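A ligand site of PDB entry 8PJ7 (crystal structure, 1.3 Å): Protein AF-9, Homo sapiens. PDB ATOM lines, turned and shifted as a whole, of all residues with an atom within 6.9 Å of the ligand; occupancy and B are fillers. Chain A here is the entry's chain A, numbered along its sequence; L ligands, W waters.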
ATOM      1  N   THR A  24      16.813 -22.423   3.692  1.00  0.00           N
ATOM      2  CA  THR A  24      17.696 -21.382   3.124  1.00  0.00           C
ATOM      3  C   THR A  24      18.395 -21.944   1.871  1.00  0.00           C
ATOM      4  O   THR A  24      18.358 -23.162   1.646  1.00  0.00           O
ATOM      5  CB  THR A  24      18.703 -20.886   4.162  1.00  0.00           C
ATOM      6  OG1 THR A  24      19.668 -21.921   4.327  1.00  0.00           O
ATOM      7  CG2 THR A  24      18.065 -20.507   5.471  1.00  0.00           C
ATOM      8  N   VAL A  25      19.102 -21.065   1.166  1.00  0.00           N
ATOM      9  CA  VAL A  25      19.850 -21.482  -0.054  1.00  0.00           C
ATOM     10  C   VAL A  25      20.911 -22.516   0.326  1.00  0.00           C
ATOM     11  O   VAL A  25      21.183 -23.408  -0.473  1.00  0.00           O
ATOM     12  CB  VAL A  25      20.481 -20.280  -0.754  1.00  0.00           C
ATOM     13  CG1 VAL A  25      21.597 -19.655   0.063  1.00  0.00           C
ATOM     14  CG2 VAL A  25      20.970 -20.684  -2.138  1.00  0.00           C
ATOM     15  N   GLU A  26      21.441 -22.436   1.557  1.00  0.00           N
ATOM     16  CA  GLU A  26      22.483 -23.388   2.040  1.00  0.00           C
ATOM     17  C   GLU A  26      21.872 -24.737   2.377  1.00  0.00           C
ATOM     18  O   GLU A  26      22.614 -25.695   2.569  1.00  0.00           O
ATOM     19  CB  GLU A  26      23.204 -22.893   3.278  1.00  0.00           C
ATOM     20  CG  GLU A  26      23.882 -21.570   3.105  1.00  0.00           C
ATOM     21  CD  GLU A  26      23.056 -20.329   3.339  1.00  0.00           C
ATOM     22  OE1 GLU A  26      21.856 -20.433   3.664  1.00  0.00           O
ATOM     23  OE2 GLU A  26      23.602 -19.238   3.216  1.00  0.00           O
ATOM     24  N   PHE A  28      19.664 -24.871   5.055  1.00  0.00           N
ATOM     25  CA  PHE A  28      19.333 -24.802   6.509  1.00  0.00           C
ATOM     26  C   PHE A  28      17.837 -24.935   6.694  1.00  0.00           C
ATOM     27  O   PHE A  28      17.072 -24.147   6.093  1.00  0.00           O
ATOM     28  CB  PHE A  28      19.883 -23.533   7.157  1.00  0.00           C
ATOM     29  CG  PHE A  28      21.349 -23.301   6.987  1.00  0.00           C
ATOM     30  CD1 PHE A  28      22.211 -24.374   6.796  1.00  0.00           C
ATOM     31  CD2 PHE A  28      21.881 -22.033   6.960  1.00  0.00           C
ATOM     32  CE1 PHE A  28      23.584 -24.171   6.608  1.00  0.00           C
ATOM     33  CE2 PHE A  28      23.239 -21.834   6.763  1.00  0.00           C
ATOM     34  CZ  PHE A  28      24.080 -22.903   6.593  1.00  0.00           C
ATOM     35  N   TRP A  32      16.681 -21.169  14.948  1.00  0.00           N
ATOM     36  CA  TRP A  32      16.752 -21.432  16.387  1.00  0.00           C
ATOM     37  C   TRP A  32      17.270 -20.203  17.104  1.00  0.00           C
ATOM     38  O   TRP A  32      17.871 -19.274  16.521  1.00  0.00           O
ATOM     39  CB  TRP A  32      17.525 -22.716  16.681  1.00  0.00           C
ATOM     40  CG  TRP A  32      18.944 -22.809  16.200  1.00  0.00           C
ATOM     41  CD1 TRP A  32      19.399 -23.639  15.226  1.00  0.00           C
ATOM     42  CD2 TRP A  32      20.127 -22.201  16.774  1.00  0.00           C
ATOM     43  NE1 TRP A  32      20.758 -23.552  15.103  1.00  0.00           N
ATOM     44  CE2 TRP A  32      21.244 -22.734  16.083  1.00  0.00           C
ATOM     45  CE3 TRP A  32      20.359 -21.344  17.827  1.00  0.00           C
ATOM     46  CZ2 TRP A  32      22.541 -22.346  16.377  1.00  0.00           C
ATOM     47  CZ3 TRP A  32      21.650 -20.947  18.093  1.00  0.00           C
ATOM     48  CH2 TRP A  32      22.724 -21.477  17.402  1.00  0.00           C
ATOM     49  N   HIS A  56      28.867 -24.645  17.373  1.00  0.00           N
ATOM     50  CA  HIS A  56      29.543 -25.678  16.566  1.00  0.00           C
ATOM     51  C   HIS A  56      30.394 -24.983  15.504  1.00  0.00           C
ATOM     52  O   HIS A  56      29.980 -23.962  14.952  1.00  0.00           O
ATOM     53  CB  HIS A  56      28.485 -26.600  15.994  1.00  0.00           C
ATOM     54  CG  HIS A  56      29.033 -27.759  15.283  1.00  0.00           C
ATOM     55  ND1 HIS A  56      29.360 -27.734  13.925  1.00  0.00           N
ATOM     56  CD2 HIS A  56      29.275 -28.995  15.739  1.00  0.00           C
ATOM     57  CE1 HIS A  56      29.778 -28.947  13.611  1.00  0.00           C
ATOM     58  NE2 HIS A  56      29.764 -29.732  14.702  1.00  0.00           N
ATOM     59  N   GLU A  57      31.575 -25.541  15.182  1.00  0.00           N
ATOM     60  CA  GLU A  57      32.544 -24.840  14.332  1.00  0.00           C
ATOM     61  C   GLU A  57      32.168 -24.883  12.850  1.00  0.00           C
ATOM     62  O   GLU A  57      32.811 -24.164  12.086  1.00  0.00           O
ATOM     63  CB  GLU A  57      33.926 -25.429  14.586  1.00  0.00           C
ATOM     64  CG  GLU A  57      34.464 -25.035  15.929  1.00  0.00           C
ATOM     65  CD  GLU A  57      35.931 -25.377  16.112  1.00  0.00           C
ATOM     66  OE1 GLU A  57      36.263 -25.897  17.176  1.00  0.00           O
ATOM     67  OE2 GLU A  57      36.709 -25.111  15.187  1.00  0.00           O
ATOM     68  N   SER A  58      31.059 -25.499  12.486  1.00  0.00           N
ATOM     69  CA  SER A  58      30.440 -25.272  11.142  1.00  0.00           C
ATOM     70  C   SER A  58      29.919 -23.842  11.004  1.00  0.00           C
ATOM     71  O   SER A  58      29.765 -23.325   9.882  1.00  0.00           O
ATOM     72  CB  SER A  58      29.381 -26.268  10.887  1.00  0.00           C
ATOM     73  OG  SER A  58      28.328 -26.223  11.859  1.00  0.00           O
ATOM     74  N   PHE A  59      29.619 -23.143  12.095  1.00  0.00           N
ATOM     75  CA  PHE A  59      29.158 -21.758  12.073  1.00  0.00           C
ATOM     76  C   PHE A  59      30.334 -20.811  11.932  1.00  0.00           C
ATOM     77  O   PHE A  59      31.357 -20.967  12.589  1.00  0.00           O
ATOM     78  CB  PHE A  59      28.385 -21.398  13.348  1.00  0.00           C
ATOM     79  CG  PHE A  59      27.034 -22.045  13.440  1.00  0.00           C
ATOM     80  CD1 PHE A  59      26.842 -23.317  13.945  1.00  0.00           C
ATOM     81  CD2 PHE A  59      25.943 -21.339  12.991  1.00  0.00           C
ATOM     82  CE1 PHE A  59      25.581 -23.885  13.957  1.00  0.00           C
ATOM     83  CE2 PHE A  59      24.683 -21.878  13.055  1.00  0.00           C
ATOM     84  CZ  PHE A  59      24.499 -23.151  13.515  1.00  0.00           C
ATOM     85  N   PRO A  60      30.153 -19.726  11.169  1.00  0.00           N
ATOM     86  CA  PRO A  60      31.175 -18.692  11.140  1.00  0.00           C
ATOM     87  C   PRO A  60      31.247 -17.969  12.500  1.00  0.00           C
ATOM     88  O   PRO A  60      30.217 -17.820  13.197  1.00  0.00           O
ATOM     89  CB  PRO A  60      30.696 -17.715  10.064  1.00  0.00           C
ATOM     90  CG  PRO A  60      29.280 -18.083   9.749  1.00  0.00           C
ATOM     91  CD  PRO A  60      28.969 -19.426  10.375  1.00  0.00           C
ATOM     92  N   ARG A  61      32.452 -17.554  12.849  1.00  0.00           N
ATOM     93  CA  ARG A  61      32.715 -16.749  14.057  1.00  0.00           C
ATOM     94  C   ARG A  61      31.943 -17.371  15.215  1.00  0.00           C
ATOM     95  O   ARG A  61      31.117 -16.712  15.843  1.00  0.00           O
ATOM     96  CB  ARG A  61      32.259 -15.302  13.885  1.00  0.00           C
ATOM     97  CG  ARG A  61      32.734 -14.552  12.649  1.00  0.00           C
ATOM     98  CD  ARG A  61      31.822 -13.329  12.448  1.00  0.00           C
ATOM     99  NE  ARG A  61      30.467 -13.662  11.941  1.00  0.00           N
ATOM    100  CZ  ARG A  61      29.305 -13.614  12.616  1.00  0.00           C
ATOM    101  NH1 ARG A  61      29.248 -13.242  13.886  1.00  0.00           N
ATOM    102  NH2 ARG A  61      28.179 -13.958  11.997  1.00  0.00           N
ATOM    103  N   ARG A  64      30.211 -16.373  20.176  1.00  0.00           N
ATOM    104  CA  ARG A  64      29.239 -15.268  20.179  1.00  0.00           C
ATOM    105  C   ARG A  64      29.218 -14.704  21.594  1.00  0.00           C
ATOM    106  O   ARG A  64      28.751 -15.376  22.535  1.00  0.00           O
ATOM    107  CB  ARG A  64      27.882 -15.785  19.705  1.00  0.00           C
ATOM    108  CG  ARG A  64      27.911 -16.473  18.360  1.00  0.00           C
ATOM    109  CD  ARG A  64      28.203 -15.521  17.219  1.00  0.00           C
ATOM    110  NE  ARG A  64      28.341 -16.259  15.968  1.00  0.00           N
ATOM    111  CZ  ARG A  64      27.323 -16.616  15.150  1.00  0.00           C
ATOM    112  NH1 ARG A  64      27.586 -17.352  14.091  1.00  0.00           N
ATOM    113  NH2 ARG A  64      26.089 -16.285  15.438  1.00  0.00           N
ATOM    114  N   GLU A  74      20.603 -15.837  17.708  1.00  0.00           N
ATOM    115  CA  GLU A  74      19.613 -16.263  16.710  1.00  0.00           C
ATOM    116  C   GLU A  74      20.348 -16.796  15.498  1.00  0.00           C
ATOM    117  O   GLU A  74      21.230 -16.046  14.989  1.00  0.00           O
ATOM    118  CB  GLU A  74      18.707 -15.131  16.274  1.00  0.00           C
ATOM    119  CG  GLU A  74      17.811 -14.578  17.374  1.00  0.00           C
ATOM    120  CD  GLU A  74      16.882 -13.505  16.845  1.00  0.00           C
ATOM    121  OE1 GLU A  74      17.367 -12.379  16.646  1.00  0.00           O
ATOM    122  OE2 GLU A  74      15.701 -13.827  16.593  1.00  0.00           O
ATOM    123  N   GLU A  75      20.088 -18.012  15.080  1.00  0.00           N
ATOM    124  CA  GLU A  75      20.782 -18.646  13.959  1.00  0.00           C
ATOM    125  C   GLU A  75      19.798 -19.445  13.135  1.00  0.00           C
ATOM    126  O   GLU A  75      18.621 -19.642  13.500  1.00  0.00           O
ATOM    127  CB  GLU A  75      21.905 -19.529  14.472  1.00  0.00           C
ATOM    128  CG  GLU A  75      23.217 -18.779  14.472  1.00  0.00           C
ATOM    129  CD  GLU A  75      23.719 -18.373  13.117  1.00  0.00           C
ATOM    130  OE1 GLU A  75      23.161 -18.789  12.109  1.00  0.00           O
ATOM    131  OE2 GLU A  75      24.673 -17.579  13.086  1.00  0.00           O
ATOM    132  N   SER A  76      20.314 -19.945  12.033  1.00  0.00           N
ATOM    133  CA  SER A  76      19.665 -20.989  11.226  1.00  0.00           C
ATOM    134  C   SER A  76      20.657 -22.137  11.075  1.00  0.00           C
ATOM    135  O   SER A  76      21.880 -21.902  11.089  1.00  0.00           O
ATOM    136  CB  SER A  76      19.210 -20.456   9.882  1.00  0.00           C
ATOM    137  OG  SER A  76      18.268 -19.426  10.029  1.00  0.00           O
ATOM    138  N   GLY A  77      20.120 -23.319  10.848  1.00  0.00           N
ATOM    139  CA  GLY A  77      20.957 -24.484  10.593  1.00  0.00           C
ATOM    140  C   GLY A  77      20.155 -25.718  10.375  1.00  0.00           C
ATOM    141  O   GLY A  77      18.944 -25.650  10.136  1.00  0.00           O
ATOM    142  N   TYR A  78      20.825 -26.875  10.451  1.00  0.00           N
ATOM    143  CA  TYR A  78      20.145 -28.120  10.066  1.00  0.00           C
ATOM    144  C   TYR A  78      20.419 -29.272  11.037  1.00  0.00           C
ATOM    145  O   TYR A  78      19.915 -30.357  10.812  1.00  0.00           O
ATOM    146  CB  TYR A  78      20.550 -28.539   8.646  1.00  0.00           C
ATOM    147  CG  TYR A  78      21.978 -28.913   8.447  1.00  0.00           C
ATOM    148  CD1 TYR A  78      22.949 -28.003   8.145  1.00  0.00           C
ATOM    149  CD2 TYR A  78      22.328 -30.243   8.497  1.00  0.00           C
ATOM    150  CE1 TYR A  78      24.244 -28.395   7.855  1.00  0.00           C
ATOM    151  CE2 TYR A  78      23.628 -30.655   8.275  1.00  0.00           C
ATOM    152  CZ  TYR A  78      24.580 -29.730   7.896  1.00  0.00           C
ATOM    153  OH  TYR A  78      25.869 -30.069   7.657  1.00  0.00           O
ATOM    154  N   ALA A  79      21.129 -29.035  12.132  1.00  0.00           N
ATOM    155  CA  ALA A  79      21.343 -30.122  13.113  1.00  0.00           C
ATOM    156  C   ALA A  79      21.573 -29.478  14.480  1.00  0.00           C
ATOM    157  O   ALA A  79      22.151 -28.389  14.575  1.00  0.00           O
ATOM    158  CB  ALA A  79      22.531 -30.955  12.749  1.00  0.00           C
ATOM    159  N   GLY A  80      21.126 -30.187  15.488  1.00  0.00           N
ATOM    160  CA  GLY A  80      21.387 -29.779  16.871  1.00  0.00           C
ATOM    161  C   GLY A  80      22.777 -30.162  17.319  1.00  0.00           C
ATOM    162  O   GLY A  80      23.508 -30.903  16.635  1.00  0.00           O
ATOM    163  N   PHE A  81      23.129 -29.691  18.506  1.00  0.00           N
ATOM    164  CA  PHE A  81      24.468 -29.932  19.058  1.00  0.00           C
ATOM    165  C   PHE A  81      24.476 -29.472  20.508  1.00  0.00           C
ATOM    166  O   PHE A  81      23.583 -28.769  20.975  1.00  0.00           O
ATOM    167  CB  PHE A  81      25.557 -29.238  18.223  1.00  0.00           C
ATOM    168  CG  PHE A  81      25.415 -27.740  18.088  1.00  0.00           C
ATOM    169  CD1 PHE A  81      24.586 -27.205  17.114  1.00  0.00           C
ATOM    170  CD2 PHE A  81      26.067 -26.888  18.956  1.00  0.00           C
ATOM    171  CE1 PHE A  81      24.409 -25.826  17.023  1.00  0.00           C
ATOM    172  CE2 PHE A  81      25.897 -25.526  18.852  1.00  0.00           C
ATOM    173  CZ  PHE A  81      25.102 -25.016  17.879  1.00  0.00           C
ATOM    174  N   LEU A 106      16.965 -30.066  17.980  1.00  0.00           N
ATOM    175  CA  LEU A 106      16.002 -29.687  16.945  1.00  0.00           C
ATOM    176  C   LEU A 106      14.998 -30.824  16.779  1.00  0.00           C
ATOM    177  O   LEU A 106      15.424 -32.038  16.900  1.00  0.00           O
ATOM    178  CB  LEU A 106      16.677 -29.477  15.606  1.00  0.00           C
ATOM    179  CG  LEU A 106      17.852 -28.524  15.564  1.00  0.00           C
ATOM    180  CD1 LEU A 106      18.318 -28.420  14.114  1.00  0.00           C
ATOM    181  CD2 LEU A 106      17.535 -27.185  16.172  1.00  0.00           C
HETATM  182  C1  LIG L   1      25.400 -27.833  13.721  1.00  0.00           C
HETATM  183  C2  LIG L   1      25.796 -29.208  14.277  1.00  0.00           C
HETATM  184  C3  LIG L   1      26.381 -29.895  13.152  1.00  0.00           C
HETATM  185  C4  LIG L   1      27.094 -31.059  13.162  1.00  0.00           C
HETATM  186  C5  LIG L   1      27.595 -31.589  11.974  1.00  0.00           C
HETATM  187  C6  LIG L   1      27.400 -30.922  10.780  1.00  0.00           C
HETATM  188  C7  LIG L   1      26.645 -29.737  10.805  1.00  0.00           C
HETATM  189  C8  LIG L   1      26.148 -29.252  11.984  1.00  0.00           C
HETATM  190  C9  LIG L   1      25.432 -28.061  12.256  1.00  0.00           C
HETATM  191  N1  LIG L   1      25.665 -26.927  11.392  1.00  0.00           N
HETATM  192  C10 LIG L   1      24.749 -25.982  10.969  1.00  0.00           C
HETATM  193  O1  LIG L   1      23.533 -26.144  11.246  1.00  0.00           O
HETATM  194  C11 LIG L   1      25.277 -24.864  10.281  1.00  0.00           C
HETATM  195  C12 LIG L   1      24.805 -23.585  10.170  1.00  0.00           C
HETATM  196  N2  LIG L   1      26.386 -24.955   9.654  1.00  0.00           N
HETATM  197  O2  LIG L   1      26.652 -23.623   9.149  1.00  0.00           O
HETATM  198  C13 LIG L   1      25.663 -22.788   9.451  1.00  0.00           C
HETATM  199  C14 LIG L   1      25.657 -21.480   9.077  1.00  0.00           C
HETATM  200  C15 LIG L   1      24.817 -20.542   9.653  1.00  0.00           C
HETATM  201  C16 LIG L   1      24.805 -19.210   9.277  1.00  0.00           C
HETATM  202  O3  LIG L   1      23.987 -18.279   9.799  1.00  0.00           O
HETATM  203  C17 LIG L   1      26.610 -20.983   8.136  1.00  0.00           C
HETATM  204  C18 LIG L   1      26.554 -19.676   7.740  1.00  0.00           C
HETATM  205  C19 LIG L   1      25.715 -18.740   8.282  1.00  0.00           C
HETATM  206  C20 LIG L   1      25.812 -17.363   7.869  1.00  0.00           C
HETATM  207  O4  LIG L   1      26.295 -16.530   8.657  1.00  0.00           O
HETATM  208  N3  LIG L   1      25.404 -16.996   6.638  1.00  0.00           N
HETATM  209  C21 LIG L   1      24.839 -17.954   5.691  1.00  0.00           C
HETATM  210  C22 LIG L   1      25.567 -15.552   6.278  1.00  0.00           C
HETATM  211  O   HOH W   1      26.431 -16.807  11.329  1.00  0.00           O
HETATM  212  O   HOH W   2      22.161 -25.777  13.692  1.00  0.00           O
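The side-chain carboxylate (OE1) of Glu 75 is in hydrogen-bond range of an oxygen (O3) of the ligand (2.5 Å). The backbone NH of Tyr 78 is in hydrogen-bond range of an oxygen (O1) of the ligand, at 2.9 Å. The side-chain hydroxyl (OG) of Ser 58 is in hydrogen-bond range of a nitrogen (N1) of the ligand (2.8 Å).
Water W1 lies within hydrogen-bond range of the side-chain carboxylate of Glu 75 (2.6 Å), an oxygen (O4) of the ligand (2.7 Å), the guanidinium group of Arg 64 (3.0 Å) and the guanidinium group of Arg 61 (3.4 Å). Water W2 lies within hydrogen-bond range of O of Ala 79 (2.8 Å), O1 of the ligand (2.8 Å) and NE1 of Trp 32 (3.0 Å).
OE2 of Glu 26 touches C21 of the ligand, at 3.1 Å. Phe 28 touches the ligand. His 56 touches the ligand. Phe 59 touches the ligand (CE2 to C12, 3.4 Å). CG of Pro 60 touches O4 of the ligand, at 3.5 Å. O of Ser 76 touches C12 of the ligand, at 3.5 Å. Gly 77 touches the ligand (CA to O1, 3.1 Å). Ala 79 touches the ligand. Gly 80 touches the ligand (O to C2, 3.7 Å). CD1 of Phe 81 touches C1 of the ligand (3.5 Å). Hydrophobic or aromatic side chains within 4 Å of the ligand: Phe 28, His 56, Phe 59, Pro 60, Tyr 78 and Phe 81. Along chain A the residues within 4 Å of the ligand span positions 26 to 81.
OE1 of Glu 26 is in hydrogen-bond range of OG1 of Thr 24 (2.7 Å). The side-chain carboxylate of Glu 75 is in salt-bridge range of the guanidinium group of Arg 64 (3.0 Å). O of Pro 60 is in hydrogen-bond range of NH1 of Arg 64 (2.8 Å). The backbone carbonyl oxygen of Glu 75 sits at hydrogen-bond distance from the backbone NH of Trp 32 (2.9 Å). The side-chain hydroxyl (OG) of Ser 58 is in hydrogen-bond range of a ring nitrogen (ND1) of His 56. OG1 of Thr 24 is in hydrogen-bond range of N of Phe 28, at 3.0 Å.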
